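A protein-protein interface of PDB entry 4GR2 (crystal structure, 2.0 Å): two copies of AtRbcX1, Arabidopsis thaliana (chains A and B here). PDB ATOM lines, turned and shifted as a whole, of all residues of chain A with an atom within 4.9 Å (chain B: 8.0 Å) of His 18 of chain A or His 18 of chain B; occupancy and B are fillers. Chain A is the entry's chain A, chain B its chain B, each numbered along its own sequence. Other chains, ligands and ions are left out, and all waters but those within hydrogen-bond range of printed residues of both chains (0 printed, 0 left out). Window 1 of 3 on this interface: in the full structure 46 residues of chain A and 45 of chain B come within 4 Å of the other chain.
The side-chain amide nitrogen (ND2) of Asn 103 of chain B is in hydrogen-bond range of the backbone carbonyl oxygen (O) of Ala 16 of chain A (3.3 Å).
ND2 of Asn 103 of chain B lies close to N of Lys 17 of chain A (3.4 Å).
ND1 of His 18 of chain A lies within hydrogen-bond range of NE2 of His 18 of chain B, 3.0 Å away.
The side-chain amino group (NZ) of Lys 17 of chain A is in salt-bridge range of the side-chain carboxylate (OD2) of Asp 21 of chain A, at 3.8 Å.
Tyr 25 of chain B touches Lys 14 of chain A (OH to NZ, 3.6 Å).
Ala 16 of chain A touches Ala 100 of chain B (CB to N, 3.6 Å).
His 20 of chain A touches Asn 103 of chain B (CB to CB, 3.8 Å).
Phe 22 of chain A touches Pro 11 of chain B (CZ to O, 3.4 Å).
Printed residues of chain B within 4 Å of Ala 16 of chain A: Ala 100 (3.6 Å) and Asn 103 (3.3 Å).
Of the printed residues of chain B, Lys 17 of chain A touches Asn 103 (3.4 Å).
Printed residues of chain B within 4 Å of His 18 of chain A: His 18 (3.0 Å).
Of the printed residues of chain B, His 20 of chain A touches Asn 103 (3.8 Å).
Of the printed residues of chain A, His 18 of chain B touches His 18.
Of the printed residues of chain A, Tyr 25 of chain B touches Lys 14 (3.6 Å).
The nearest printed residue of chain B that does not touch His 18 of chain A is Asn 103 of chain B (5.8 Å).
Of the 9 printed residues of chain A, 6 touch a printed residue of chain B.
Printed residues of chain A that touch a printed residue of chain B: Lys 14, Ala 16, Lys 17, His 18, His 20 and Phe 22.
Among the printed residues, no Asp or Glu carboxylate lies within 4 Å of a Lys or Arg side-chain nitrogen of the other chain.
His 18 of chain A touches its own counterpart, His 18 of chain B.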
ATOM      1  N   LYS A  14       8.052   8.613  28.899  1.00  0.00           N
ATOM      2  CA  LYS A  14       7.119   7.892  29.759  1.00  0.00           C
ATOM      3  C   LYS A  14       6.556   6.697  29.012  1.00  0.00           C
ATOM      4  O   LYS A  14       6.427   5.614  29.568  1.00  0.00           O
ATOM      5  CB  LYS A  14       5.991   8.822  30.200  1.00  0.00           C
ATOM      6  CG  LYS A  14       6.377   9.723  31.372  1.00  0.00           C
ATOM      7  CD  LYS A  14       5.234  10.640  31.782  1.00  0.00           C
ATOM      8  CE  LYS A  14       5.712  11.713  32.749  1.00  0.00           C
ATOM      9  NZ  LYS A  14       4.655  12.727  32.986  1.00  0.00           N
ATOM     10  N   ALA A  15       6.235   6.911  27.736  1.00  0.00           N
ATOM     11  CA  ALA A  15       5.692   5.862  26.893  1.00  0.00           C
ATOM     12  C   ALA A  15       6.703   4.724  26.692  1.00  0.00           C
ATOM     13  O   ALA A  15       6.332   3.549  26.713  1.00  0.00           O
ATOM     14  CB  ALA A  15       5.281   6.438  25.547  1.00  0.00           C
ATOM     15  N   ALA A  16       7.964   5.100  26.474  1.00  0.00           N
ATOM     16  CA  ALA A  16       9.077   4.155  26.354  1.00  0.00           C
ATOM     17  C   ALA A  16       9.318   3.303  27.606  1.00  0.00           C
ATOM     18  O   ALA A  16       9.615   2.118  27.487  1.00  0.00           O
ATOM     19  CB  ALA A  16      10.371   4.901  25.951  1.00  0.00           C
ATOM     20  N   LYS A  17       9.219   3.896  28.800  1.00  0.00           N
ATOM     21  CA  LYS A  17       9.358   3.114  30.043  1.00  0.00           C
ATOM     22  C   LYS A  17       8.262   2.059  30.134  1.00  0.00           C
ATOM     23  O   LYS A  17       8.522   0.896  30.488  1.00  0.00           O
ATOM     24  CB  LYS A  17       9.309   4.008  31.286  1.00  0.00           C
ATOM     25  CG  LYS A  17       9.326   3.227  32.623  1.00  0.00           C
ATOM     26  CD  LYS A  17      10.489   2.206  32.694  1.00  0.00           C
ATOM     27  CE  LYS A  17      10.418   1.289  33.948  1.00  0.00           C
ATOM     28  NZ  LYS A  17      10.014   2.087  35.157  1.00  0.00           N
ATOM     29  N   HIS A  18       7.033   2.463  29.819  1.00  0.00           N
ATOM     30  CA  HIS A  18       5.899   1.539  29.802  1.00  0.00           C
ATOM     31  C   HIS A  18       6.073   0.421  28.785  1.00  0.00           C
ATOM     32  O   HIS A  18       5.666  -0.716  29.018  1.00  0.00           O
ATOM     33  CB  HIS A  18       4.572   2.259  29.518  1.00  0.00           C
ATOM     34  CG  HIS A  18       3.370   1.456  29.914  1.00  0.00           C
ATOM     35  ND1 HIS A  18       2.584   0.781  29.004  1.00  0.00           N
ATOM     36  CD2 HIS A  18       2.838   1.197  31.133  1.00  0.00           C
ATOM     37  CE1 HIS A  18       1.616   0.149  29.646  1.00  0.00           C
ATOM     38  NE2 HIS A  18       1.748   0.386  30.937  1.00  0.00           N
ATOM     39  N   LEU A  19       6.655   0.752  27.639  1.00  0.00           N
ATOM     40  CA  LEU A  19       6.835  -0.260  26.607  1.00  0.00           C
ATOM     41  C   LEU A  19       7.926  -1.270  26.994  1.00  0.00           C
ATOM     42  O   LEU A  19       7.829  -2.444  26.653  1.00  0.00           O
ATOM     43  CB  LEU A  19       7.151   0.377  25.263  1.00  0.00           C
ATOM     44  CG  LEU A  19       5.954   0.942  24.512  1.00  0.00           C
ATOM     45  CD1 LEU A  19       6.420   1.733  23.300  1.00  0.00           C
ATOM     46  CD2 LEU A  19       4.998  -0.192  24.089  1.00  0.00           C
ATOM     47  N   HIS A  20       8.966  -0.788  27.669  1.00  0.00           N
ATOM     48  CA  HIS A  20      10.030  -1.647  28.198  1.00  0.00           C
ATOM     49  C   HIS A  20       9.407  -2.704  29.128  1.00  0.00           C
ATOM     50  O   HIS A  20       9.644  -3.887  28.971  1.00  0.00           O
ATOM     51  CB  HIS A  20      11.064  -0.762  28.914  1.00  0.00           C
ATOM     52  CG  HIS A  20      11.990  -1.490  29.839  1.00  0.00           C
ATOM     53  ND1 HIS A  20      12.638  -0.854  30.875  1.00  0.00           N
ATOM     54  CD2 HIS A  20      12.401  -2.780  29.877  1.00  0.00           C
ATOM     55  CE1 HIS A  20      13.403  -1.717  31.515  1.00  0.00           C
ATOM     56  NE2 HIS A  20      13.261  -2.899  30.942  1.00  0.00           N
ATOM     57  N   ASP A  21       8.560  -2.281  30.063  1.00  0.00           N
ATOM     58  CA  ASP A  21       7.965  -3.246  30.982  1.00  0.00           C
ATOM     59  C   ASP A  21       6.957  -4.145  30.291  1.00  0.00           C
ATOM     60  O   ASP A  21       6.802  -5.309  30.633  1.00  0.00           O
ATOM     61  CB  ASP A  21       7.356  -2.530  32.175  1.00  0.00           C
ATOM     62  CG  ASP A  21       8.417  -1.950  33.066  1.00  0.00           C
ATOM     63  OD1 ASP A  21       9.543  -2.529  33.119  1.00  0.00           O
ATOM     64  OD2 ASP A  21       8.142  -0.922  33.711  1.00  0.00           O
ATOM     65  N   PHE A  22       6.270  -3.578  29.315  1.00  0.00           N
ATOM     66  CA  PHE A  22       5.327  -4.307  28.484  1.00  0.00           C
ATOM     67  C   PHE A  22       6.060  -5.421  27.714  1.00  0.00           C
ATOM     68  O   PHE A  22       5.563  -6.539  27.609  1.00  0.00           O
ATOM     69  CB  PHE A  22       4.642  -3.312  27.525  1.00  0.00           C
ATOM     70  CG  PHE A  22       3.728  -3.954  26.535  1.00  0.00           C
ATOM     71  CD1 PHE A  22       2.562  -4.585  26.955  1.00  0.00           C
ATOM     72  CD2 PHE A  22       4.030  -3.936  25.189  1.00  0.00           C
ATOM     73  CE1 PHE A  22       1.711  -5.182  26.046  1.00  0.00           C
ATOM     74  CE2 PHE A  22       3.189  -4.552  24.266  1.00  0.00           C
ATOM     75  CZ  PHE A  22       2.030  -5.168  24.701  1.00  0.00           C
ATOM     76  N   PRO B  11      -0.122  -7.948  20.768  1.00  0.00           N
ATOM     77  CA  PRO B  11       0.614  -6.978  21.585  1.00  0.00           C
ATOM     78  C   PRO B  11       0.508  -5.572  21.010  1.00  0.00           C
ATOM     79  O   PRO B  11       0.466  -4.617  21.780  1.00  0.00           O
ATOM     80  CB  PRO B  11       2.053  -7.481  21.502  1.00  0.00           C
ATOM     81  CG  PRO B  11       1.910  -8.975  21.316  1.00  0.00           C
ATOM     82  CD  PRO B  11       0.705  -9.126  20.428  1.00  0.00           C
ATOM     83  N   GLU B  12       0.472  -5.442  19.683  1.00  0.00           N
ATOM     84  CA  GLU B  12       0.335  -4.123  19.063  1.00  0.00           C
ATOM     85  C   GLU B  12      -0.986  -3.446  19.437  1.00  0.00           C
ATOM     86  O   GLU B  12      -1.029  -2.231  19.733  1.00  0.00           O
ATOM     87  CB  GLU B  12       0.478  -4.247  17.554  1.00  0.00           C
ATOM     88  CG  GLU B  12       1.890  -4.624  17.121  1.00  0.00           C
ATOM     89  CD  GLU B  12       2.143  -6.119  17.057  1.00  0.00           C
ATOM     90  OE1 GLU B  12       1.240  -6.916  17.410  1.00  0.00           O
ATOM     91  OE2 GLU B  12       3.265  -6.497  16.629  1.00  0.00           O
ATOM     92  N   ALA B  13      -2.070  -4.220  19.424  1.00  0.00           N
ATOM     93  CA  ALA B  13      -3.383  -3.649  19.740  1.00  0.00           C
ATOM     94  C   ALA B  13      -3.419  -3.279  21.202  1.00  0.00           C
ATOM     95  O   ALA B  13      -3.980  -2.256  21.573  1.00  0.00           O
ATOM     96  CB  ALA B  13      -4.520  -4.629  19.414  1.00  0.00           C
ATOM     97  N   LYS B  14      -2.796  -4.106  22.041  1.00  0.00           N
ATOM     98  CA  LYS B  14      -2.729  -3.804  23.468  1.00  0.00           C
ATOM     99  C   LYS B  14      -1.969  -2.511  23.705  1.00  0.00           C
ATOM    100  O   LYS B  14      -2.430  -1.642  24.446  1.00  0.00           O
ATOM    101  CB  LYS B  14      -2.096  -4.967  24.256  1.00  0.00           C
ATOM    102  CG  LYS B  14      -2.980  -6.231  24.326  1.00  0.00           C
ATOM    103  CD  LYS B  14      -2.157  -7.491  24.633  1.00  0.00           C
ATOM    104  CE  LYS B  14      -2.615  -8.221  25.890  1.00  0.00           C
ATOM    105  NZ  LYS B  14      -3.979  -8.801  25.740  1.00  0.00           N
ATOM    106  N   ALA B  15      -0.800  -2.395  23.082  1.00  0.00           N
ATOM    107  CA  ALA B  15       0.011  -1.191  23.205  1.00  0.00           C
ATOM    108  C   ALA B  15      -0.753   0.012  22.656  1.00  0.00           C
ATOM    109  O   ALA B  15      -0.680   1.118  23.214  1.00  0.00           O
ATOM    110  CB  ALA B  15       1.302  -1.364  22.429  1.00  0.00           C
ATOM    111  N   ALA B  16      -1.457  -0.219  21.549  1.00  0.00           N
ATOM    112  CA  ALA B  16      -2.269   0.813  20.880  1.00  0.00           C
ATOM    113  C   ALA B  16      -3.365   1.415  21.781  1.00  0.00           C
ATOM    114  O   ALA B  16      -3.583   2.640  21.799  1.00  0.00           O
ATOM    115  CB  ALA B  16      -2.890   0.220  19.637  1.00  0.00           C
ATOM    116  N   LYS B  17      -4.050   0.550  22.529  1.00  0.00           N
ATOM    117  CA  LYS B  17      -5.083   0.982  23.479  1.00  0.00           C
ATOM    118  C   LYS B  17      -4.457   1.732  24.653  1.00  0.00           C
ATOM    119  O   LYS B  17      -5.021   2.701  25.142  1.00  0.00           O
ATOM    120  CB  LYS B  17      -5.882  -0.224  24.002  1.00  0.00           C
ATOM    121  CG  LYS B  17      -7.033   0.163  24.965  1.00  0.00           C
ATOM    122  CD  LYS B  17      -8.171   0.924  24.240  1.00  0.00           C
ATOM    123  CE  LYS B  17      -9.052   1.719  25.224  1.00  0.00           C
ATOM    124  NZ  LYS B  17      -9.294   0.976  26.506  1.00  0.00           N
ATOM    125  N   HIS B  18      -3.304   1.271  25.132  1.00  0.00           N
ATOM    126  CA  HIS B  18      -2.577   2.002  26.174  1.00  0.00           C
ATOM    127  C   HIS B  18      -2.150   3.387  25.706  1.00  0.00           C
ATOM    128  O   HIS B  18      -2.260   4.357  26.453  1.00  0.00           O
ATOM    129  CB  HIS B  18      -1.331   1.250  26.686  1.00  0.00           C
ATOM    130  CG  HIS B  18      -0.576   2.014  27.734  1.00  0.00           C
ATOM    131  ND1 HIS B  18      -1.073   2.223  29.002  1.00  0.00           N
ATOM    132  CD2 HIS B  18       0.612   2.661  27.687  1.00  0.00           C
ATOM    133  CE1 HIS B  18      -0.211   2.943  29.701  1.00  0.00           C
ATOM    134  NE2 HIS B  18       0.819   3.223  28.925  1.00  0.00           N
ATOM    135  N   LEU B  19      -1.660   3.492  24.467  1.00  0.00           N
ATOM    136  CA  LEU B  19      -1.297   4.805  23.924  1.00  0.00           C
ATOM    137  C   LEU B  19      -2.523   5.742  23.819  1.00  0.00           C
ATOM    138  O   LEU B  19      -2.477   6.897  24.253  1.00  0.00           O
ATOM    139  CB  LEU B  19      -0.590   4.655  22.574  1.00  0.00           C
ATOM    140  CG  LEU B  19       0.836   4.129  22.801  1.00  0.00           C
ATOM    141  CD1 LEU B  19       1.446   3.657  21.484  1.00  0.00           C
ATOM    142  CD2 LEU B  19       1.698   5.211  23.475  1.00  0.00           C
ATOM    143  N   HIS B  20      -3.616   5.211  23.277  1.00  0.00           N
ATOM    144  CA  HIS B  20      -4.892   5.944  23.189  1.00  0.00           C
ATOM    145  C   HIS B  20      -5.217   6.617  24.535  1.00  0.00           C
ATOM    146  O   HIS B  20      -5.364   7.842  24.618  1.00  0.00           O
ATOM    147  CB  HIS B  20      -6.004   4.978  22.727  1.00  0.00           C
ATOM    148  CG  HIS B  20      -7.379   5.583  22.715  1.00  0.00           C
ATOM    149  ND1 HIS B  20      -8.446   5.022  23.387  1.00  0.00           N
ATOM    150  CD2 HIS B  20      -7.862   6.691  22.108  1.00  0.00           C
ATOM    151  CE1 HIS B  20      -9.523   5.762  23.205  1.00  0.00           C
ATOM    152  NE2 HIS B  20      -9.194   6.785  22.437  1.00  0.00           N
ATOM    153  N   ASP B  21      -5.257   5.814  25.599  1.00  0.00           N
ATOM    154  CA  ASP B  21      -5.540   6.332  26.931  1.00  0.00           C
ATOM    155  C   ASP B  21      -4.467   7.290  27.397  1.00  0.00           C
ATOM    156  O   ASP B  21      -4.777   8.316  28.019  1.00  0.00           O
ATOM    157  CB  ASP B  21      -5.733   5.199  27.958  1.00  0.00           C
ATOM    158  CG  ASP B  21      -7.062   4.483  27.793  1.00  0.00           C
ATOM    159  OD1 ASP B  21      -8.048   5.147  27.375  1.00  0.00           O
ATOM    160  OD2 ASP B  21      -7.116   3.261  28.080  1.00  0.00           O
ATOM    161  N   PHE B  22      -3.209   6.956  27.118  1.00  0.00           N
ATOM    162  CA  PHE B  22      -2.105   7.872  27.422  1.00  0.00           C
ATOM    163  C   PHE B  22      -2.301   9.238  26.715  1.00  0.00           C
ATOM    164  O   PHE B  22      -2.077  10.283  27.311  1.00  0.00           O
ATOM    165  CB  PHE B  22      -0.742   7.255  27.045  1.00  0.00           C
ATOM    166  CG  PHE B  22       0.435   8.096  27.467  1.00  0.00           C
ATOM    167  CD1 PHE B  22       0.612   8.441  28.808  1.00  0.00           C
ATOM    168  CD2 PHE B  22       1.347   8.571  26.527  1.00  0.00           C
ATOM    169  CE1 PHE B  22       1.691   9.235  29.205  1.00  0.00           C
ATOM    170  CE2 PHE B  22       2.430   9.361  26.920  1.00  0.00           C
ATOM    171  CZ  PHE B  22       2.602   9.692  28.242  1.00  0.00           C
ATOM    172  N   PHE B  23      -2.710   9.216  25.447  1.00  0.00           N
ATOM    173  CA  PHE B  23      -2.940  10.466  24.703  1.00  0.00           C
ATOM    174  C   PHE B  23      -4.083  11.291  25.275  1.00  0.00           C
ATOM    175  O   PHE B  23      -3.994  12.522  25.318  1.00  0.00           O
ATOM    176  CB  PHE B  23      -3.159  10.200  23.211  1.00  0.00           C
ATOM    177  CG  PHE B  23      -1.937   9.673  22.513  1.00  0.00           C
ATOM    178  CD1 PHE B  23      -0.680  10.115  22.882  1.00  0.00           C
ATOM    179  CD2 PHE B  23      -2.046   8.702  21.524  1.00  0.00           C
ATOM    180  CE1 PHE B  23       0.463   9.618  22.248  1.00  0.00           C
ATOM    181  CE2 PHE B  23      -0.909   8.187  20.893  1.00  0.00           C
ATOM    182  CZ  PHE B  23       0.346   8.656  21.260  1.00  0.00           C
ATOM    183  N   THR B  24      -5.144  10.628  25.728  1.00  0.00           N
ATOM    184  CA  THR B  24      -6.223  11.334  26.451  1.00  0.00           C
ATOM    185  C   THR B  24      -5.690  12.065  27.661  1.00  0.00           C
ATOM    186  O   THR B  24      -6.064  13.196  27.923  1.00  0.00           O
ATOM    187  CB  THR B  24      -7.317  10.375  26.924  1.00  0.00           C
ATOM    188  OG1 THR B  24      -7.855   9.679  25.788  1.00  0.00           O
ATOM    189  CG2 THR B  24      -8.436  11.120  27.689  1.00  0.00           C
ATOM    190  N   TYR B  25      -4.782  11.420  28.390  1.00  0.00           N
ATOM    191  CA  TYR B  25      -4.187  12.008  29.583  1.00  0.00           C
ATOM    192  C   TYR B  25      -3.248  13.181  29.266  1.00  0.00           C
ATOM    193  O   TYR B  25      -3.264  14.193  29.970  1.00  0.00           O
ATOM    194  CB  TYR B  25      -3.468  10.929  30.422  1.00  0.00           C
ATOM    195  CG  TYR B  25      -2.272  11.444  31.189  1.00  0.00           C
ATOM    196  CD1 TYR B  25      -2.404  11.952  32.478  1.00  0.00           C
ATOM    197  CD2 TYR B  25      -1.003  11.432  30.614  1.00  0.00           C
ATOM    198  CE1 TYR B  25      -1.297  12.434  33.172  1.00  0.00           C
ATOM    199  CE2 TYR B  25       0.099  11.914  31.293  1.00  0.00           C
ATOM    200  CZ  TYR B  25      -0.051  12.409  32.572  1.00  0.00           C
ATOM    201  OH  TYR B  25       1.063  12.880  33.232  1.00  0.00           O
ATOM    202  N   SER B  56      -8.212   7.526  33.918  1.00  0.00           N
ATOM    203  CA  SER B  56      -7.672   6.176  33.631  1.00  0.00           C
ATOM    204  C   SER B  56      -8.325   5.369  32.479  1.00  0.00           C
ATOM    205  O   SER B  56      -7.645   5.038  31.496  1.00  0.00           O
ATOM    206  CB  SER B  56      -7.557   5.359  34.912  1.00  0.00           C
ATOM    207  OG  SER B  56      -6.536   5.910  35.740  1.00  0.00           O
ATOM    208  N   ALA B 100      12.717   3.282  23.806  1.00  0.00           N
ATOM    209  CA  ALA B 100      12.285   1.978  24.298  1.00  0.00           C
ATOM    210  C   ALA B 100      13.385   0.963  24.047  1.00  0.00           C
ATOM    211  O   ALA B 100      13.640   0.081  24.880  1.00  0.00           O
ATOM    212  CB  ALA B 100      11.007   1.542  23.605  1.00  0.00           C
ATOM    213  N   ASN B 103      15.995   1.644  26.532  1.00  0.00           N
ATOM    214  CA  ASN B 103      15.590   1.139  27.844  1.00  0.00           C
ATOM    215  C   ASN B 103      15.835  -0.366  27.955  1.00  0.00           C
ATOM    216  O   ASN B 103      16.336  -0.854  28.962  1.00  0.00           O
ATOM    217  CB  ASN B 103      14.101   1.426  28.108  1.00  0.00           C
ATOM    218  CG  ASN B 103      13.840   2.866  28.519  1.00  0.00           C
ATOM    219  OD1 ASN B 103      14.744   3.568  28.958  1.00  0.00           O
ATOM    220  ND2 ASN B 103      12.585   3.308  28.393  1.00  0.00           N
